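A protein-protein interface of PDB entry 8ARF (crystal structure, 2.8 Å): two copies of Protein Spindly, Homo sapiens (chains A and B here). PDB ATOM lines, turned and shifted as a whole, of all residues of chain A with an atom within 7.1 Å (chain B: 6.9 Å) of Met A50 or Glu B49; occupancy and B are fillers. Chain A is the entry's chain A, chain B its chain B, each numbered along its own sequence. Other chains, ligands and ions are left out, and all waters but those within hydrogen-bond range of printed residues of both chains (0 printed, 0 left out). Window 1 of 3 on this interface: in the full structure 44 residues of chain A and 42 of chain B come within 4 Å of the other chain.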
ATOM      1  N   ASP A  44     -15.814  31.569 -26.093  1.00  0.00           N
ATOM      2  CA  ASP A  44     -15.517  30.675 -27.222  1.00  0.00           C
ATOM      3  C   ASP A  44     -16.216  29.325 -27.080  1.00  0.00           C
ATOM      4  O   ASP A  44     -16.836  28.873 -28.035  1.00  0.00           O
ATOM      5  CB  ASP A  44     -14.018  30.525 -27.436  1.00  0.00           C
ATOM      6  CG  ASP A  44     -13.418  31.741 -28.132  1.00  0.00           C
ATOM      7  OD1 ASP A  44     -14.157  32.720 -28.418  1.00  0.00           O
ATOM      8  OD2 ASP A  44     -12.204  31.697 -28.428  1.00  0.00           O
ATOM      9  N   LYS A  45     -16.152  28.725 -25.884  1.00  0.00           N
ATOM     10  CA  LYS A  45     -16.880  27.485 -25.569  1.00  0.00           C
ATOM     11  C   LYS A  45     -18.362  27.592 -25.925  1.00  0.00           C
ATOM     12  O   LYS A  45     -18.830  26.840 -26.747  1.00  0.00           O
ATOM     13  CB  LYS A  45     -16.689  27.098 -24.106  1.00  0.00           C
ATOM     14  CG  LYS A  45     -17.471  25.885 -23.624  1.00  0.00           C
ATOM     15  CD  LYS A  45     -17.191  25.625 -22.135  1.00  0.00           C
ATOM     16  CE  LYS A  45     -16.688  24.201 -21.890  1.00  0.00           C
ATOM     17  NZ  LYS A  45     -15.272  24.049 -22.375  1.00  0.00           N
ATOM     18  N   CYS A  46     -19.055  28.566 -25.332  1.00  0.00           N
ATOM     19  CA  CYS A  46     -20.456  28.853 -25.594  1.00  0.00           C
ATOM     20  C   CYS A  46     -20.692  28.904 -27.105  1.00  0.00           C
ATOM     21  O   CYS A  46     -21.540  28.198 -27.620  1.00  0.00           O
ATOM     22  CB  CYS A  46     -20.865  30.197 -24.937  1.00  0.00           C
ATOM     23  SG  CYS A  46     -22.612  30.820 -25.134  1.00  0.00           S
ATOM     24  N   ARG A  47     -19.933  29.759 -27.793  1.00  0.00           N
ATOM     25  CA  ARG A  47     -20.133  30.014 -29.185  1.00  0.00           C
ATOM     26  C   ARG A  47     -19.948  28.669 -29.973  1.00  0.00           C
ATOM     27  O   ARG A  47     -20.647  28.400 -30.959  1.00  0.00           O
ATOM     28  CB  ARG A  47     -19.144  31.060 -29.640  1.00  0.00           C
ATOM     29  CG  ARG A  47     -19.625  32.041 -30.686  1.00  0.00           C
ATOM     30  CD  ARG A  47     -19.052  33.429 -30.440  1.00  0.00           C
ATOM     31  NE  ARG A  47     -20.047  34.230 -29.727  1.00  0.00           N
ATOM     32  CZ  ARG A  47     -20.085  35.560 -29.692  1.00  0.00           C
ATOM     33  NH1 ARG A  47     -19.166  36.270 -30.343  1.00  0.00           N
ATOM     34  NH2 ARG A  47     -21.046  36.182 -29.003  1.00  0.00           N
ATOM     35  N   ASN A  48     -18.981  27.851 -29.559  1.00  0.00           N
ATOM     36  CA  ASN A  48     -18.749  26.593 -30.229  1.00  0.00           C
ATOM     37  C   ASN A  48     -19.917  25.646 -30.017  1.00  0.00           C
ATOM     38  O   ASN A  48     -20.519  25.180 -30.986  1.00  0.00           O
ATOM     39  CB  ASN A  48     -17.457  25.926 -29.775  1.00  0.00           C
ATOM     40  CG  ASN A  48     -16.988  24.883 -30.783  1.00  0.00           C
ATOM     41  OD1 ASN A  48     -16.717  25.209 -31.936  1.00  0.00           O
ATOM     42  ND2 ASN A  48     -16.949  23.626 -30.376  1.00  0.00           N
ATOM     43  N   GLU A  49     -20.257  25.408 -28.744  1.00  0.00           N
ATOM     44  CA  GLU A  49     -21.480  24.639 -28.369  1.00  0.00           C
ATOM     45  C   GLU A  49     -22.719  25.040 -29.141  1.00  0.00           C
ATOM     46  O   GLU A  49     -23.453  24.162 -29.538  1.00  0.00           O
ATOM     47  CB  GLU A  49     -21.823  24.785 -26.892  1.00  0.00           C
ATOM     48  CG  GLU A  49     -20.824  24.110 -25.968  1.00  0.00           C
ATOM     49  CD  GLU A  49     -21.065  24.447 -24.508  1.00  0.00           C
ATOM     50  OE1 GLU A  49     -21.163  25.659 -24.218  1.00  0.00           O
ATOM     51  OE2 GLU A  49     -21.149  23.507 -23.672  1.00  0.00           O
ATOM     52  N   MET A  50     -22.908  26.349 -29.365  1.00  0.00           N
ATOM     53  CA  MET A  50     -23.996  26.868 -30.179  1.00  0.00           C
ATOM     54  C   MET A  50     -23.930  26.331 -31.587  1.00  0.00           C
ATOM     55  O   MET A  50     -24.885  25.715 -32.065  1.00  0.00           O
ATOM     56  CB  MET A  50     -24.050  28.372 -30.247  1.00  0.00           C
ATOM     57  CG  MET A  50     -25.474  28.880 -30.412  1.00  0.00           C
ATOM     58  SD  MET A  50     -25.914  30.430 -29.592  1.00  0.00           S
ATOM     59  CE  MET A  50     -24.872  31.518 -30.597  1.00  0.00           C
ATOM     60  N   MET A  51     -22.785  26.500 -32.233  1.00  0.00           N
ATOM     61  CA  MET A  51     -22.643  26.077 -33.616  1.00  0.00           C
ATOM     62  C   MET A  51     -22.900  24.605 -33.784  1.00  0.00           C
ATOM     63  O   MET A  51     -23.635  24.220 -34.679  1.00  0.00           O
ATOM     64  CB  MET A  51     -21.277  26.459 -34.192  1.00  0.00           C
ATOM     65  CG  MET A  51     -21.208  27.945 -34.592  1.00  0.00           C
ATOM     66  SD  MET A  51     -22.846  28.773 -34.806  1.00  0.00           S
ATOM     67  CE  MET A  51     -22.644  30.180 -33.691  1.00  0.00           C
ATOM     68  N   THR A  52     -22.292  23.792 -32.919  1.00  0.00           N
ATOM     69  CA  THR A  52     -22.461  22.358 -32.981  1.00  0.00           C
ATOM     70  C   THR A  52     -23.963  21.995 -32.819  1.00  0.00           C
ATOM     71  O   THR A  52     -24.515  21.266 -33.669  1.00  0.00           O
ATOM     72  CB  THR A  52     -21.616  21.593 -31.968  1.00  0.00           C
ATOM     73  OG1 THR A  52     -22.212  21.729 -30.674  1.00  0.00           O
ATOM     74  CG2 THR A  52     -20.169  22.132 -31.959  1.00  0.00           C
ATOM     75  N   MET A  53     -24.624  22.542 -31.787  1.00  0.00           N
ATOM     76  CA  MET A  53     -26.038  22.323 -31.572  1.00  0.00           C
ATOM     77  C   MET A  53     -26.811  22.720 -32.812  1.00  0.00           C
ATOM     78  O   MET A  53     -27.507  21.898 -33.375  1.00  0.00           O
ATOM     79  CB  MET A  53     -26.493  23.108 -30.356  1.00  0.00           C
ATOM     80  CG  MET A  53     -28.000  23.370 -30.219  1.00  0.00           C
ATOM     81  SD  MET A  53     -28.465  25.145 -30.322  1.00  0.00           S
ATOM     82  CE  MET A  53     -27.651  25.793 -28.884  1.00  0.00           C
ATOM     83  N   THR A  54     -26.678  23.958 -33.264  1.00  0.00           N
ATOM     84  CA  THR A  54     -27.372  24.422 -34.471  1.00  0.00           C
ATOM     85  C   THR A  54     -27.201  23.487 -35.680  1.00  0.00           C
ATOM     86  O   THR A  54     -28.142  23.079 -36.294  1.00  0.00           O
ATOM     87  CB  THR A  54     -26.922  25.846 -34.830  1.00  0.00           C
ATOM     88  OG1 THR A  54     -27.372  26.727 -33.783  1.00  0.00           O
ATOM     89  CG2 THR A  54     -27.478  26.344 -36.178  1.00  0.00           C
ATOM     90  N   GLU A  55     -25.977  23.064 -35.949  1.00  0.00           N
ATOM     91  CA  GLU A  55     -25.737  22.115 -37.016  1.00  0.00           C
ATOM     92  C   GLU A  55     -26.457  20.791 -36.735  1.00  0.00           C
ATOM     93  O   GLU A  55     -27.190  20.294 -37.565  1.00  0.00           O
ATOM     94  CB  GLU A  55     -24.234  21.877 -37.163  1.00  0.00           C
ATOM     95  CG  GLU A  55     -23.822  20.641 -37.938  1.00  0.00           C
ATOM     96  CD  GLU A  55     -22.908  19.735 -37.114  1.00  0.00           C
ATOM     97  OE1 GLU A  55     -23.150  19.528 -35.876  1.00  0.00           O
ATOM     98  OE2 GLU A  55     -21.949  19.202 -37.734  1.00  0.00           O
ATOM     99  N   SER A  56     -26.235  20.216 -35.559  1.00  0.00           N
ATOM    100  CA  SER A  56     -26.857  18.939 -35.231  1.00  0.00           C
ATOM    101  C   SER A  56     -28.370  18.967 -35.129  1.00  0.00           C
ATOM    102  O   SER A  56     -29.015  17.918 -35.140  1.00  0.00           O
ATOM    103  CB  SER A  56     -26.335  18.360 -33.927  1.00  0.00           C
ATOM    104  OG  SER A  56     -27.128  18.835 -32.867  1.00  0.00           O
ATOM    105  N   GLN B  42     -21.659  40.005 -23.345  1.00  0.00           N
ATOM    106  CA  GLN B  42     -21.900  39.205 -24.542  1.00  0.00           C
ATOM    107  C   GLN B  42     -21.859  37.705 -24.237  1.00  0.00           C
ATOM    108  O   GLN B  42     -22.401  36.937 -24.966  1.00  0.00           O
ATOM    109  CB  GLN B  42     -20.996  39.617 -25.686  1.00  0.00           C
ATOM    110  CG  GLN B  42     -19.642  38.943 -25.696  1.00  0.00           C
ATOM    111  CD  GLN B  42     -18.686  39.571 -26.716  1.00  0.00           C
ATOM    112  OE1 GLN B  42     -18.471  40.789 -26.731  1.00  0.00           O
ATOM    113  NE2 GLN B  42     -18.101  38.733 -27.572  1.00  0.00           N
ATOM    114  N   ASP B  44     -23.194  36.592 -21.320  1.00  0.00           N
ATOM    115  CA  ASP B  44     -24.549  36.495 -20.797  1.00  0.00           C
ATOM    116  C   ASP B  44     -25.546  36.422 -21.960  1.00  0.00           C
ATOM    117  O   ASP B  44     -26.503  35.645 -21.917  1.00  0.00           O
ATOM    118  CB  ASP B  44     -24.861  37.676 -19.882  1.00  0.00           C
ATOM    119  CG  ASP B  44     -23.904  37.754 -18.678  1.00  0.00           C
ATOM    120  OD1 ASP B  44     -23.377  36.678 -18.273  1.00  0.00           O
ATOM    121  OD2 ASP B  44     -23.661  38.877 -18.147  1.00  0.00           O
ATOM    122  N   LYS B  45     -25.295  37.205 -23.011  1.00  0.00           N
ATOM    123  CA  LYS B  45     -26.137  37.205 -24.193  1.00  0.00           C
ATOM    124  C   LYS B  45     -26.049  35.860 -24.930  1.00  0.00           C
ATOM    125  O   LYS B  45     -27.049  35.319 -25.378  1.00  0.00           O
ATOM    126  CB  LYS B  45     -25.752  38.331 -25.140  1.00  0.00           C
ATOM    127  CG  LYS B  45     -26.905  39.237 -25.577  1.00  0.00           C
ATOM    128  CD  LYS B  45     -27.270  39.058 -27.069  1.00  0.00           C
ATOM    129  CE  LYS B  45     -26.100  39.308 -28.029  1.00  0.00           C
ATOM    130  NZ  LYS B  45     -26.055  40.728 -28.448  1.00  0.00           N
ATOM    131  N   CYS B  46     -24.843  35.315 -25.063  1.00  0.00           N
ATOM    132  CA  CYS B  46     -24.659  34.018 -25.671  1.00  0.00           C
ATOM    133  C   CYS B  46     -25.470  32.942 -24.912  1.00  0.00           C
ATOM    134  O   CYS B  46     -26.203  32.159 -25.524  1.00  0.00           O
ATOM    135  CB  CYS B  46     -23.174  33.672 -25.749  1.00  0.00           C
ATOM    136  SG  CYS B  46     -22.660  32.210 -26.713  1.00  0.00           S
ATOM    137  N   ARG B  47     -25.334  32.901 -23.589  1.00  0.00           N
ATOM    138  CA  ARG B  47     -26.063  31.919 -22.810  1.00  0.00           C
ATOM    139  C   ARG B  47     -27.593  32.020 -22.975  1.00  0.00           C
ATOM    140  O   ARG B  47     -28.276  31.007 -22.895  1.00  0.00           O
ATOM    141  CB  ARG B  47     -25.686  31.992 -21.332  1.00  0.00           C
ATOM    142  CG  ARG B  47     -24.638  30.977 -20.879  1.00  0.00           C
ATOM    143  CD  ARG B  47     -23.202  31.562 -20.908  1.00  0.00           C
ATOM    144  NE  ARG B  47     -22.176  30.767 -20.223  1.00  0.00           N
ATOM    145  CZ  ARG B  47     -21.575  31.086 -19.068  1.00  0.00           C
ATOM    146  NH1 ARG B  47     -21.890  32.197 -18.389  1.00  0.00           N
ATOM    147  NH2 ARG B  47     -20.654  30.272 -18.559  1.00  0.00           N
ATOM    148  N   ASN B  48     -28.106  33.246 -23.175  1.00  0.00           N
ATOM    149  CA  ASN B  48     -29.536  33.506 -23.341  1.00  0.00           C
ATOM    150  C   ASN B  48     -30.012  32.964 -24.653  1.00  0.00           C
ATOM    151  O   ASN B  48     -31.004  32.235 -24.679  1.00  0.00           O
ATOM    152  CB  ASN B  48     -29.880  35.007 -23.336  1.00  0.00           C
ATOM    153  CG  ASN B  48     -30.081  35.558 -21.957  1.00  0.00           C
ATOM    154  OD1 ASN B  48     -30.754  34.934 -21.154  1.00  0.00           O
ATOM    155  ND2 ASN B  48     -29.524  36.736 -21.680  1.00  0.00           N
ATOM    156  N   GLU B  49     -29.331  33.353 -25.737  1.00  0.00           N
ATOM    157  CA  GLU B  49     -29.749  32.930 -27.068  1.00  0.00           C
ATOM    158  C   GLU B  49     -29.563  31.404 -27.264  1.00  0.00           C
ATOM    159  O   GLU B  49     -30.176  30.823 -28.132  1.00  0.00           O
ATOM    160  CB  GLU B  49     -29.046  33.731 -28.144  1.00  0.00           C
ATOM    161  CG  GLU B  49     -27.566  33.435 -28.271  1.00  0.00           C
ATOM    162  CD  GLU B  49     -26.700  34.647 -28.678  1.00  0.00           C
ATOM    163  OE1 GLU B  49     -25.466  34.444 -28.916  1.00  0.00           O
ATOM    164  OE2 GLU B  49     -27.224  35.789 -28.732  1.00  0.00           O
ATOM    165  N   MET B  50     -28.731  30.778 -26.429  1.00  0.00           N
ATOM    166  CA  MET B  50     -28.585  29.344 -26.435  1.00  0.00           C
ATOM    167  C   MET B  50     -29.830  28.656 -25.932  1.00  0.00           C
ATOM    168  O   MET B  50     -30.322  27.734 -26.544  1.00  0.00           O
ATOM    169  CB  MET B  50     -27.395  28.911 -25.570  1.00  0.00           C
ATOM    170  CG  MET B  50     -26.677  27.673 -26.094  1.00  0.00           C
ATOM    171  SD  MET B  50     -25.099  27.918 -27.050  1.00  0.00           S
ATOM    172  CE  MET B  50     -23.972  27.191 -25.871  1.00  0.00           C
ATOM    173  N   MET B  51     -30.352  29.141 -24.811  1.00  0.00           N
ATOM    174  CA  MET B  51     -31.581  28.618 -24.229  1.00  0.00           C
ATOM    175  C   MET B  51     -32.756  28.855 -25.135  1.00  0.00           C
ATOM    176  O   MET B  51     -33.560  27.922 -25.371  1.00  0.00           O
ATOM    177  CB  MET B  51     -31.858  29.207 -22.830  1.00  0.00           C
ATOM    178  CG  MET B  51     -30.942  28.655 -21.747  1.00  0.00           C
ATOM    179  SD  MET B  51     -30.225  27.042 -22.229  1.00  0.00           S
ATOM    180  CE  MET B  51     -28.453  27.297 -22.032  1.00  0.00           C
ATOM    181  N   THR B  52     -32.867  30.086 -25.645  1.00  0.00           N
ATOM    182  CA  THR B  52     -33.904  30.426 -26.618  1.00  0.00           C
ATOM    183  C   THR B  52     -33.873  29.474 -27.813  1.00  0.00           C
ATOM    184  O   THR B  52     -34.909  28.911 -28.189  1.00  0.00           O
ATOM    185  CB  THR B  52     -33.688  31.826 -27.139  1.00  0.00           C
ATOM    186  OG1 THR B  52     -33.598  32.685 -26.002  1.00  0.00           O
ATOM    187  CG2 THR B  52     -34.812  32.303 -28.069  1.00  0.00           C
ATOM    188  N   MET B  53     -32.671  29.277 -28.372  1.00  0.00           N
ATOM    189  CA  MET B  53     -32.493  28.395 -29.496  1.00  0.00           C
ATOM    190  C   MET B  53     -32.933  27.009 -29.141  1.00  0.00           C
ATOM    191  O   MET B  53     -33.672  26.383 -29.881  1.00  0.00           O
ATOM    192  CB  MET B  53     -31.029  28.311 -29.904  1.00  0.00           C
ATOM    193  CG  MET B  53     -30.777  28.401 -31.390  1.00  0.00           C
ATOM    194  SD  MET B  53     -29.105  28.905 -31.697  1.00  0.00           S
ATOM    195  CE  MET B  53     -29.374  30.708 -31.714  1.00  0.00           C
ATOM    196  N   THR B  54     -32.422  26.479 -28.037  1.00  0.00           N
ATOM    197  CA  THR B  54     -32.709  25.093 -27.681  1.00  0.00           C
ATOM    198  C   THR B  54     -34.222  24.844 -27.642  1.00  0.00           C
ATOM    199  O   THR B  54     -34.708  23.930 -28.318  1.00  0.00           O
ATOM    200  CB  THR B  54     -32.007  24.647 -26.410  1.00  0.00           C
ATOM    201  OG1 THR B  54     -30.609  24.746 -26.638  1.00  0.00           O
ATOM    202  CG2 THR B  54     -32.225  23.209 -26.153  1.00  0.00           C
ATOM    203  N   TYR B  57     -35.694  24.883 -31.156  1.00  0.00           N
ATOM    204  CA  TYR B  57     -35.364  23.698 -31.899  1.00  0.00           C
ATOM    205  C   TYR B  57     -36.154  22.510 -31.426  1.00  0.00           C
ATOM    206  O   TYR B  57     -36.584  21.700 -32.227  1.00  0.00           O
ATOM    207  CB  TYR B  57     -33.849  23.408 -31.849  1.00  0.00           C
ATOM    208  CG  TYR B  57     -33.078  24.293 -32.810  1.00  0.00           C
ATOM    209  CD1 TYR B  57     -33.686  24.833 -33.933  1.00  0.00           C
ATOM    210  CD2 TYR B  57     -31.757  24.593 -32.601  1.00  0.00           C
ATOM    211  CE1 TYR B  57     -33.001  25.644 -34.804  1.00  0.00           C
ATOM    212  CE2 TYR B  57     -31.058  25.415 -33.471  1.00  0.00           C
ATOM    213  CZ  TYR B  57     -31.694  25.943 -34.576  1.00  0.00           C
ATOM    214  OH  TYR B  57     -31.045  26.764 -35.482  1.00  0.00           O
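Of the 13 printed residues of chain B, 8 touch a printed residue of chain A. Hydrophobic or aromatic side chains of chain B that line the printed part of chain A: Met B50, Met B53 and Tyr B57. Printed residues of chain A that touch a printed residue of chain B: Cys A46, Arg A47, Glu A49, Met A50, Met A53 and Thr A54. Among the printed residues, no Asp or Glu carboxylate lies within 4 Å of a Lys or Arg side-chain nitrogen of the other chain.
The side-chain sulfur (SG) of Cys B46 is disulfide-bonded to the side-chain sulfur (SG) of Cys A46 (2.1 Å). The side-chain sulfur of Met B50 lies close to the backbone NH of Met A50, at 3.6 Å. The backbone carbonyl oxygen (O) of Cys A46 lies close to the side-chain sulfur (SD) of Met B50 (3.6 Å). N of Arg B47 is in hydrogen-bond range of SG of Cys A46, 3.8 Å away. The side-chain sulfur (SD) of Met B53 lies within hydrogen-bond range of the side-chain hydroxyl (OG1) of Thr A54 (3.5 Å).
Cys A46 touches Met B50, but with the chains exchanged Met A50 does not touch Cys B46 (4.4 Å). Glu A49 touches Met B50, and with the chains exchanged Met A50 touches Glu B49. Met A50 touches Met B53, and with the chains exchanged Met A53 touches Met B50. Met A53 touches Thr B54, and with the chains exchanged Thr A54 touches Met B53.
Gln B42 touches Arg A47 (NE2 to NH1, 3.9 Å). Cys B46 touches Arg A47. CB of Glu A49 touches CE of Met B50, 3.4 Å away. Met A50 touches Glu B49 (CE to OE1, 3.4 Å). SD of Met B53 touches CG of Met A50, 3.9 Å away. Met A53 touches Met B50 (CE to CG, 3.5 Å). Met A53 touches Thr B54. OH of Tyr B57 touches CG2 of Thr A54, at 3.7 Å.
The backbone carbonyl oxygen (O) of Met A50 sits at hydrogen-bond distance from the side-chain hydroxyl (OG1) of Thr A54. The backbone carbonyl oxygen (O) of Glu A49 lies within hydrogen-bond range of the side-chain hydroxyl (OG1) of Thr A52 (3.0 Å). OG1 of Thr B54 is in hydrogen-bond range of O of Met B50, at 3.0 Å. O of Met A53 is in hydrogen-bond range of OG of Ser A56, at 3.1 Å.
Met A50 touches just these residues of chain B: Glu B49 (3.4 Å), Met B50 (3.4 Å) and Met B53 (3.9 Å). Glu B49 touches one residue of chain A. Printed residues of chain A within 4 Å of Tyr B57: Thr A54. Of the printed residues of chain A, Cys B46 touches Cys A46 (2.1 Å) and Arg A47 (3.8 Å). Of the printed residues of chain A, Gln B42 touches Arg A47. Printed residues of chain A within 4 Å of Met B50: Cys A46 (3.2 Å), Glu A49 (3.4 Å), Met A50 (3.4 Å) and Met A53 (3.5 Å). Printed residues of chain B within 4 Å of Arg A47: Gln B42 and Cys B46. Asp B44 touches none of the printed residues of chain A. The nearest residue of chain B that does not touch Met A50 is Cys B46 (4.4 Å).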
